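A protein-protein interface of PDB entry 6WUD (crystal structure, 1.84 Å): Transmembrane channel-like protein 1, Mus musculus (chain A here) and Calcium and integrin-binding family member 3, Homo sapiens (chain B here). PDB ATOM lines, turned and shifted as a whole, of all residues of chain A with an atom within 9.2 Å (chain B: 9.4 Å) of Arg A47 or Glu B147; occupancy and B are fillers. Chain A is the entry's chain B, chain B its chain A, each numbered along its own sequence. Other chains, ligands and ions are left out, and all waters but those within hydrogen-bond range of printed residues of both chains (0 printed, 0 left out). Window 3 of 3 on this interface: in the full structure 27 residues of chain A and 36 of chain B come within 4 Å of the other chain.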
ATOM      1  N   PHE A  10     -31.638 -29.677   1.080  1.00  0.00           N
ATOM      2  CA  PHE A  10     -32.430 -28.569   1.612  1.00  0.00           C
ATOM      3  C   PHE A  10     -33.562 -28.184   0.665  1.00  0.00           C
ATOM      4  O   PHE A  10     -34.669 -27.822   1.108  1.00  0.00           O
ATOM      5  CB  PHE A  10     -31.522 -27.375   1.871  1.00  0.00           C
ATOM      6  CG  PHE A  10     -30.622 -27.539   3.073  1.00  0.00           C
ATOM      7  CD1 PHE A  10     -29.440 -28.275   2.997  1.00  0.00           C
ATOM      8  CD2 PHE A  10     -30.961 -26.947   4.278  1.00  0.00           C
ATOM      9  CE1 PHE A  10     -28.617 -28.413   4.103  1.00  0.00           C
ATOM     10  CE2 PHE A  10     -30.120 -27.060   5.389  1.00  0.00           C
ATOM     11  CZ  PHE A  10     -28.962 -27.806   5.301  1.00  0.00           C
ATOM     12  N   PHE A  39     -35.216 -29.148  10.041  1.00  0.00           N
ATOM     13  CA  PHE A  39     -34.295 -28.115   9.558  1.00  0.00           C
ATOM     14  C   PHE A  39     -33.117 -27.931  10.520  1.00  0.00           C
ATOM     15  O   PHE A  39     -31.964 -27.757  10.098  1.00  0.00           O
ATOM     16  CB  PHE A  39     -35.029 -26.779   9.367  1.00  0.00           C
ATOM     17  CG  PHE A  39     -35.690 -26.620   8.017  1.00  0.00           C
ATOM     18  CD1 PHE A  39     -34.935 -26.553   6.858  1.00  0.00           C
ATOM     19  CD2 PHE A  39     -37.060 -26.532   7.921  1.00  0.00           C
ATOM     20  CE1 PHE A  39     -35.550 -26.409   5.616  1.00  0.00           C
ATOM     21  CE2 PHE A  39     -37.688 -26.395   6.692  1.00  0.00           C
ATOM     22  CZ  PHE A  39     -36.926 -26.317   5.528  1.00  0.00           C
ATOM     23  N   LYS A  40     -33.379 -27.937  11.825  1.00  0.00           N
ATOM     24  CA  LYS A  40     -32.287 -27.754  12.790  1.00  0.00           C
ATOM     25  C   LYS A  40     -31.269 -28.892  12.705  1.00  0.00           C
ATOM     26  O   LYS A  40     -30.071 -28.650  12.669  1.00  0.00           O
ATOM     27  CB  LYS A  40     -32.840 -27.595  14.202  1.00  0.00           C
ATOM     28  CG  LYS A  40     -33.553 -26.270  14.402  1.00  0.00           C
ATOM     29  CD  LYS A  40     -34.010 -26.080  15.836  1.00  0.00           C
ATOM     30  CE  LYS A  40     -34.601 -24.696  16.045  1.00  0.00           C
ATOM     31  NZ  LYS A  40     -34.992 -24.472  17.463  1.00  0.00           N
ATOM     32  N   GLU A  41     -31.749 -30.125  12.643  1.00  0.00           N
ATOM     33  CA  GLU A  41     -30.877 -31.279  12.437  1.00  0.00           C
ATOM     34  C   GLU A  41     -30.040 -31.115  11.171  1.00  0.00           C
ATOM     35  O   GLU A  41     -28.818 -31.309  11.183  1.00  0.00           O
ATOM     36  CB  GLU A  41     -31.733 -32.553  12.372  1.00  0.00           C
ATOM     37  CG  GLU A  41     -32.476 -32.925  13.661  1.00  0.00           C
ATOM     38  CD  GLU A  41     -31.538 -33.118  14.856  1.00  0.00           C
ATOM     39  OE1 GLU A  41     -30.445 -33.704  14.666  1.00  0.00           O
ATOM     40  OE2 GLU A  41     -31.897 -32.695  15.979  1.00  0.00           O
ATOM     41  N   ALA A  42     -30.684 -30.758  10.065  1.00  0.00           N
ATOM     42  CA  ALA A  42     -29.956 -30.626   8.807  1.00  0.00           C
ATOM     43  C   ALA A  42     -28.913 -29.517   8.878  1.00  0.00           C
ATOM     44  O   ALA A  42     -27.807 -29.650   8.330  1.00  0.00           O
ATOM     45  CB  ALA A  42     -30.931 -30.362   7.672  1.00  0.00           C
ATOM     46  N   ILE A  43     -29.261 -28.427   9.544  1.00  0.00           N
ATOM     47  CA  ILE A  43     -28.341 -27.316   9.703  1.00  0.00           C
ATOM     48  C   ILE A  43     -27.121 -27.750  10.517  1.00  0.00           C
ATOM     49  O   ILE A  43     -25.996 -27.374  10.206  1.00  0.00           O
ATOM     50  CB  ILE A  43     -29.024 -26.124  10.383  1.00  0.00           C
ATOM     51  CG1 ILE A  43     -30.044 -25.501   9.431  1.00  0.00           C
ATOM     52  CG2 ILE A  43     -27.994 -25.096  10.807  1.00  0.00           C
ATOM     53  CD1 ILE A  43     -30.708 -24.258   9.972  1.00  0.00           C
ATOM     54  N   ILE A  44     -27.355 -28.549  11.554  1.00  0.00           N
ATOM     55  CA  ILE A  44     -26.274 -29.048  12.397  1.00  0.00           C
ATOM     56  C   ILE A  44     -25.319 -29.910  11.580  1.00  0.00           C
ATOM     57  O   ILE A  44     -24.107 -29.746  11.656  1.00  0.00           O
ATOM     58  CB  ILE A  44     -26.810 -29.904  13.556  1.00  0.00           C
ATOM     59  CG1 ILE A  44     -27.601 -29.040  14.534  1.00  0.00           C
ATOM     60  CG2 ILE A  44     -25.667 -30.597  14.275  1.00  0.00           C
ATOM     61  CD1 ILE A  44     -26.947 -27.710  14.824  1.00  0.00           C
ATOM     62  N   GLU A  45     -25.869 -30.808  10.769  1.00  0.00           N
ATOM     63  CA  GLU A  45     -25.040 -31.649   9.910  1.00  0.00           C
ATOM     64  C   GLU A  45     -24.298 -30.804   8.881  1.00  0.00           C
ATOM     65  O   GLU A  45     -23.130 -31.068   8.563  1.00  0.00           O
ATOM     66  CB  GLU A  45     -25.903 -32.714   9.218  1.00  0.00           C
ATOM     67  CG  GLU A  45     -25.954 -34.064   9.945  1.00  0.00           C
ATOM     68  CD  GLU A  45     -24.926 -35.063   9.413  1.00  0.00           C
ATOM     69  OE1 GLU A  45     -24.728 -35.108   8.179  1.00  0.00           O
ATOM     70  OE2 GLU A  45     -24.317 -35.803  10.226  1.00  0.00           O
ATOM     71  N   GLU A  46     -24.955 -29.765   8.360  1.00  0.00           N
ATOM     72  CA  GLU A  46     -24.343 -28.960   7.308  1.00  0.00           C
ATOM     73  C   GLU A  46     -23.135 -28.194   7.835  1.00  0.00           C
ATOM     74  O   GLU A  46     -22.104 -28.109   7.157  1.00  0.00           O
ATOM     75  CB  GLU A  46     -25.376 -28.007   6.715  1.00  0.00           C
ATOM     76  CG  GLU A  46     -24.893 -27.214   5.519  1.00  0.00           C
ATOM     77  CD  GLU A  46     -24.250 -28.074   4.454  1.00  0.00           C
ATOM     78  OE1 GLU A  46     -24.679 -29.232   4.274  1.00  0.00           O
ATOM     79  OE2 GLU A  46     -23.315 -27.584   3.800  1.00  0.00           O
ATOM     80  N   ARG A  47     -23.243 -27.631   9.041  1.00  0.00           N
ATOM     81  CA  ARG A  47     -22.107 -26.931   9.626  1.00  0.00           C
ATOM     82  C   ARG A  47     -20.974 -27.905   9.921  1.00  0.00           C
ATOM     83  O   ARG A  47     -19.795 -27.566   9.766  1.00  0.00           O
ATOM     84  CB  ARG A  47     -22.542 -26.205  10.893  1.00  0.00           C
ATOM     85  CG  ARG A  47     -23.240 -24.894  10.605  1.00  0.00           C
ATOM     86  CD  ARG A  47     -23.972 -24.373  11.830  1.00  0.00           C
ATOM     87  NE  ARG A  47     -24.470 -23.014  11.622  1.00  0.00           N
ATOM     88  CZ  ARG A  47     -25.455 -22.451  12.321  1.00  0.00           C
ATOM     89  NH1 ARG A  47     -26.063 -23.123  13.291  1.00  0.00           N
ATOM     90  NH2 ARG A  47     -25.838 -21.208  12.048  1.00  0.00           N
ATOM     91  N   ALA A  48     -21.314 -29.120  10.349  1.00  0.00           N
ATOM     92  CA  ALA A  48     -20.304 -30.156  10.542  1.00  0.00           C
ATOM     93  C   ALA A  48     -19.598 -30.488   9.232  1.00  0.00           C
ATOM     94  O   ALA A  48     -18.376 -30.689   9.208  1.00  0.00           O
ATOM     95  CB  ALA A  48     -20.957 -31.404  11.139  1.00  0.00           C
ATOM     96  N   ALA A  49     -20.353 -30.563   8.132  1.00  0.00           N
ATOM     97  CA  ALA A  49     -19.733 -30.749   6.824  1.00  0.00           C
ATOM     98  C   ALA A  49     -18.796 -29.592   6.498  1.00  0.00           C
ATOM     99  O   ALA A  49     -17.689 -29.802   5.990  1.00  0.00           O
ATOM    100  CB  ALA A  49     -20.808 -30.893   5.746  1.00  0.00           C
ATOM    101  N   GLN A  50     -19.222 -28.364   6.784  1.00  0.00           N
ATOM    102  CA  GLN A  50     -18.376 -27.192   6.603  1.00  0.00           C
ATOM    103  C   GLN A  50     -17.042 -27.408   7.315  1.00  0.00           C
ATOM    104  O   GLN A  50     -16.214 -26.501   7.412  1.00  0.00           O
ATOM    105  CB  GLN A  50     -19.080 -25.945   7.130  1.00  0.00           C
ATOM    106  CG  GLN A  50     -19.568 -24.993   6.050  1.00  0.00           C
ATOM    107  CD  GLN A  50     -20.312 -23.804   6.631  1.00  0.00           C
ATOM    108  OE1 GLN A  50     -20.097 -23.431   7.787  1.00  0.00           O
ATOM    109  NE2 GLN A  50     -21.196 -23.207   5.836  1.00  0.00           N
ATOM    110  N   GLU B 133     -36.926 -16.859   1.688  1.00  0.00           N
ATOM    111  CA  GLU B 133     -37.028 -16.432   3.068  1.00  0.00           C
ATOM    112  C   GLU B 133     -38.480 -16.483   3.520  1.00  0.00           C
ATOM    113  O   GLU B 133     -38.770 -16.952   4.610  1.00  0.00           O
ATOM    114  CB  GLU B 133     -36.494 -15.016   3.196  1.00  0.00           C
ATOM    115  CG  GLU B 133     -36.871 -14.313   4.481  1.00  0.00           C
ATOM    116  CD  GLU B 133     -36.114 -13.017   4.643  1.00  0.00           C
ATOM    117  OE1 GLU B 133     -36.759 -11.956   4.765  1.00  0.00           O
ATOM    118  OE2 GLU B 133     -34.868 -13.062   4.618  1.00  0.00           O
ATOM    119  N   VAL B 136     -39.500 -20.320   3.843  1.00  0.00           N
ATOM    120  CA  VAL B 136     -38.946 -20.986   5.017  1.00  0.00           C
ATOM    121  C   VAL B 136     -39.581 -20.455   6.288  1.00  0.00           C
ATOM    122  O   VAL B 136     -39.844 -21.218   7.234  1.00  0.00           O
ATOM    123  CB  VAL B 136     -37.411 -20.832   5.044  1.00  0.00           C
ATOM    124  CG1 VAL B 136     -36.862 -21.330   6.338  1.00  0.00           C
ATOM    125  CG2 VAL B 136     -36.793 -21.613   3.884  1.00  0.00           C
ATOM    126  N   THR B 137     -39.815 -19.140   6.346  1.00  0.00           N
ATOM    127  CA  THR B 137     -40.410 -18.537   7.527  1.00  0.00           C
ATOM    128  C   THR B 137     -41.799 -19.108   7.798  1.00  0.00           C
ATOM    129  O   THR B 137     -42.137 -19.457   8.937  1.00  0.00           O
ATOM    130  CB  THR B 137     -40.477 -17.022   7.351  1.00  0.00           C
ATOM    131  OG1 THR B 137     -39.142 -16.473   7.308  1.00  0.00           O
ATOM    132  CG2 THR B 137     -41.233 -16.383   8.514  1.00  0.00           C
ATOM    133  N   LEU B 144     -37.184 -20.396  13.269  1.00  0.00           N
ATOM    134  CA  LEU B 144     -35.762 -20.355  12.970  1.00  0.00           C
ATOM    135  C   LEU B 144     -35.276 -18.914  13.066  1.00  0.00           C
ATOM    136  O   LEU B 144     -36.021 -17.969  12.795  1.00  0.00           O
ATOM    137  CB  LEU B 144     -35.474 -20.905  11.578  1.00  0.00           C
ATOM    138  CG  LEU B 144     -35.824 -22.360  11.272  1.00  0.00           C
ATOM    139  CD1 LEU B 144     -35.577 -22.628   9.779  1.00  0.00           C
ATOM    140  CD2 LEU B 144     -35.023 -23.318  12.137  1.00  0.00           C
ATOM    141  N   SER B 145     -34.021 -18.749  13.453  1.00  0.00           N
ATOM    142  CA  SER B 145     -33.456 -17.411  13.509  1.00  0.00           C
ATOM    143  C   SER B 145     -33.221 -16.878  12.094  1.00  0.00           C
ATOM    144  O   SER B 145     -33.071 -17.639  11.136  1.00  0.00           O
ATOM    145  CB  SER B 145     -32.139 -17.414  14.272  1.00  0.00           C
ATOM    146  OG  SER B 145     -31.155 -18.082  13.504  1.00  0.00           O
ATOM    147  N   ALA B 146     -33.104 -15.565  11.970  1.00  0.00           N
ATOM    148  CA  ALA B 146     -32.877 -14.967  10.661  1.00  0.00           C
ATOM    149  C   ALA B 146     -31.594 -15.528  10.045  1.00  0.00           C
ATOM    150  O   ALA B 146     -31.567 -15.805   8.852  1.00  0.00           O
ATOM    151  CB  ALA B 146     -32.793 -13.458  10.779  1.00  0.00           C
ATOM    152  N   GLU B 147     -30.527 -15.671  10.827  1.00  0.00           N
ATOM    153  CA  GLU B 147     -29.317 -16.300  10.341  1.00  0.00           C
ATOM    154  C   GLU B 147     -29.558 -17.759   9.936  1.00  0.00           C
ATOM    155  O   GLU B 147     -29.017 -18.208   8.934  1.00  0.00           O
ATOM    156  CB  GLU B 147     -28.242 -16.240  11.430  1.00  0.00           C
ATOM    157  CG  GLU B 147     -26.864 -16.697  10.991  1.00  0.00           C
ATOM    158  CD  GLU B 147     -26.616 -18.165  11.260  1.00  0.00           C
ATOM    159  OE1 GLU B 147     -25.676 -18.733  10.670  1.00  0.00           O
ATOM    160  OE2 GLU B 147     -27.358 -18.751  12.070  1.00  0.00           O
ATOM    161  N   GLU B 148     -30.356 -18.485  10.712  1.00  0.00           N
ATOM    162  CA  GLU B 148     -30.649 -19.876  10.391  1.00  0.00           C
ATOM    163  C   GLU B 148     -31.384 -19.950   9.059  1.00  0.00           C
ATOM    164  O   GLU B 148     -31.091 -20.807   8.226  1.00  0.00           O
ATOM    165  CB  GLU B 148     -31.483 -20.521  11.493  1.00  0.00           C
ATOM    166  CG  GLU B 148     -30.659 -21.043  12.653  1.00  0.00           C
ATOM    167  CD  GLU B 148     -31.486 -21.823  13.648  1.00  0.00           C
ATOM    168  OE1 GLU B 148     -32.530 -21.301  14.086  1.00  0.00           O
ATOM    169  OE2 GLU B 148     -31.089 -22.951  13.993  1.00  0.00           O
ATOM    170  N   VAL B 149     -32.334 -19.046   8.860  1.00  0.00           N
ATOM    171  CA  VAL B 149     -33.056 -18.998   7.597  1.00  0.00           C
ATOM    172  C   VAL B 149     -32.093 -18.738   6.450  1.00  0.00           C
ATOM    173  O   VAL B 149     -32.197 -19.353   5.388  1.00  0.00           O
ATOM    174  CB  VAL B 149     -34.161 -17.934   7.648  1.00  0.00           C
ATOM    175  CG1 VAL B 149     -34.898 -17.859   6.314  1.00  0.00           C
ATOM    176  CG2 VAL B 149     -35.137 -18.255   8.756  1.00  0.00           C
ATOM    177  N   SER B 150     -31.131 -17.835   6.648  1.00  0.00           N
ATOM    178  CA  SER B 150     -30.230 -17.473   5.556  1.00  0.00           C
ATOM    179  C   SER B 150     -29.441 -18.674   5.063  1.00  0.00           C
ATOM    180  O   SER B 150     -29.271 -18.861   3.851  1.00  0.00           O
ATOM    181  CB  SER B 150     -29.267 -16.377   5.997  1.00  0.00           C
ATOM    182  OG  SER B 150     -29.886 -15.113   5.922  1.00  0.00           O
ATOM    183  N   LEU B 151     -28.944 -19.500   5.982  1.00  0.00           N
ATOM    184  CA  LEU B 151     -28.203 -20.686   5.567  1.00  0.00           C
ATOM    185  C   LEU B 151     -29.057 -21.573   4.674  1.00  0.00           C
ATOM    186  O   LEU B 151     -28.602 -22.038   3.619  1.00  0.00           O
ATOM    187  CB  LEU B 151     -27.722 -21.480   6.779  1.00  0.00           C
ATOM    188  CG  LEU B 151     -27.027 -22.769   6.345  1.00  0.00           C
ATOM    189  CD1 LEU B 151     -25.624 -22.444   5.778  1.00  0.00           C
ATOM    190  CD2 LEU B 151     -26.928 -23.772   7.470  1.00  0.00           C
ATOM    191  N   VAL B 152     -30.296 -21.844   5.095  1.00  0.00           N
ATOM    192  CA  VAL B 152     -31.178 -22.689   4.294  1.00  0.00           C
ATOM    193  C   VAL B 152     -31.355 -22.095   2.902  1.00  0.00           C
ATOM    194  O   VAL B 152     -31.260 -22.788   1.881  1.00  0.00           O
ATOM    195  CB  VAL B 152     -32.540 -22.868   4.987  1.00  0.00           C
ATOM    196  CG1 VAL B 152     -33.497 -23.680   4.060  1.00  0.00           C
ATOM    197  CG2 VAL B 152     -32.385 -23.527   6.331  1.00  0.00           C
ATOM    198  N   CYS B 153     -31.631 -20.797   2.842  1.00  0.00           N
ATOM    199  CA  CYS B 153     -31.894 -20.150   1.565  1.00  0.00           C
ATOM    200  C   CYS B 153     -30.684 -20.262   0.649  1.00  0.00           C
ATOM    201  O   CYS B 153     -30.819 -20.578  -0.539  1.00  0.00           O
ATOM    202  CB  CYS B 153     -32.266 -18.683   1.813  1.00  0.00           C
ATOM    203  SG  CYS B 153     -33.921 -18.453   2.560  1.00  0.00           S
ATOM    204  N   GLU B 154     -29.499 -20.039   1.211  1.00  0.00           N
ATOM    205  CA  GLU B 154     -28.269 -20.150   0.444  1.00  0.00           C
ATOM    206  C   GLU B 154     -28.051 -21.579  -0.036  1.00  0.00           C
ATOM    207  O   GLU B 154     -27.663 -21.786  -1.174  1.00  0.00           O
ATOM    208  CB  GLU B 154     -27.079 -19.649   1.257  1.00  0.00           C
ATOM    209  CG  GLU B 154     -27.081 -18.141   1.443  1.00  0.00           C
ATOM    210  CD  GLU B 154     -27.146 -17.390   0.126  1.00  0.00           C
ATOM    211  OE1 GLU B 154     -26.473 -17.814  -0.837  1.00  0.00           O
ATOM    212  OE2 GLU B 154     -27.868 -16.373   0.049  1.00  0.00           O
ATOM    213  N   LYS B 155     -28.303 -22.571   0.814  1.00  0.00           N
ATOM    214  CA  LYS B 155     -28.155 -23.935   0.375  1.00  0.00           C
ATOM    215  C   LYS B 155     -29.111 -24.309  -0.749  1.00  0.00           C
ATOM    216  O   LYS B 155     -28.732 -25.027  -1.634  1.00  0.00           O
ATOM    217  CB  LYS B 155     -28.329 -24.890   1.537  1.00  0.00           C
ATOM    218  CG  LYS B 155     -27.150 -24.899   2.478  1.00  0.00           C
ATOM    219  CD  LYS B 155     -25.907 -25.413   1.782  1.00  0.00           C
ATOM    220  CE  LYS B 155     -26.066 -26.850   1.343  1.00  0.00           C
ATOM    221  NZ  LYS B 155     -24.979 -27.287   0.429  1.00  0.00           N
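OE1 of Glu B147 is in salt-bridge range of NH2 of Arg A47 (2.8 Å).
The side-chain amino group of Lys B155 lies within salt-bridge range of the side-chain carboxylate of Glu A46 (3.8 Å).
The backbone NH (N) of Glu B148 lies within hydrogen-bond range of the side-chain hydroxyl (OG) of Ser B145, 2.9 Å away.
Among the printed residues, pairs that only touch across the chains: Phe A10 with Lys B155 (3.8 Å), Phe A39 with Val B152 (3.8 Å), Ile A43 with Glu B148 (3.9 Å) and Ile A43 with Leu B151 (3.7 Å).
Printed residues of chain B within 4 Å of Ile A43: Glu B148 (3.9 Å) and Leu B151 (3.7 Å).
Arg A47 touches just one residue of chain B: Glu B147 (2.8 Å).
No residue of chain B comes within 4 Å of Ala A48.
No residue of chain B comes within 4 Å of Ala A49.
Printed residues of chain A within 4 Å of Glu B147: Arg A47 (2.8 Å).
Printed residues of chain A within 4 Å of Glu B148: Ile A43.
Printed residues of chain A within 4 Å of Lys B155: Phe A10 and Glu A46.
Of the 13 printed residues of chain A, 5 touch a printed residue of chain B.
Along chain B the printed residues that touch a printed residue of chain A span positions 147 to 155.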
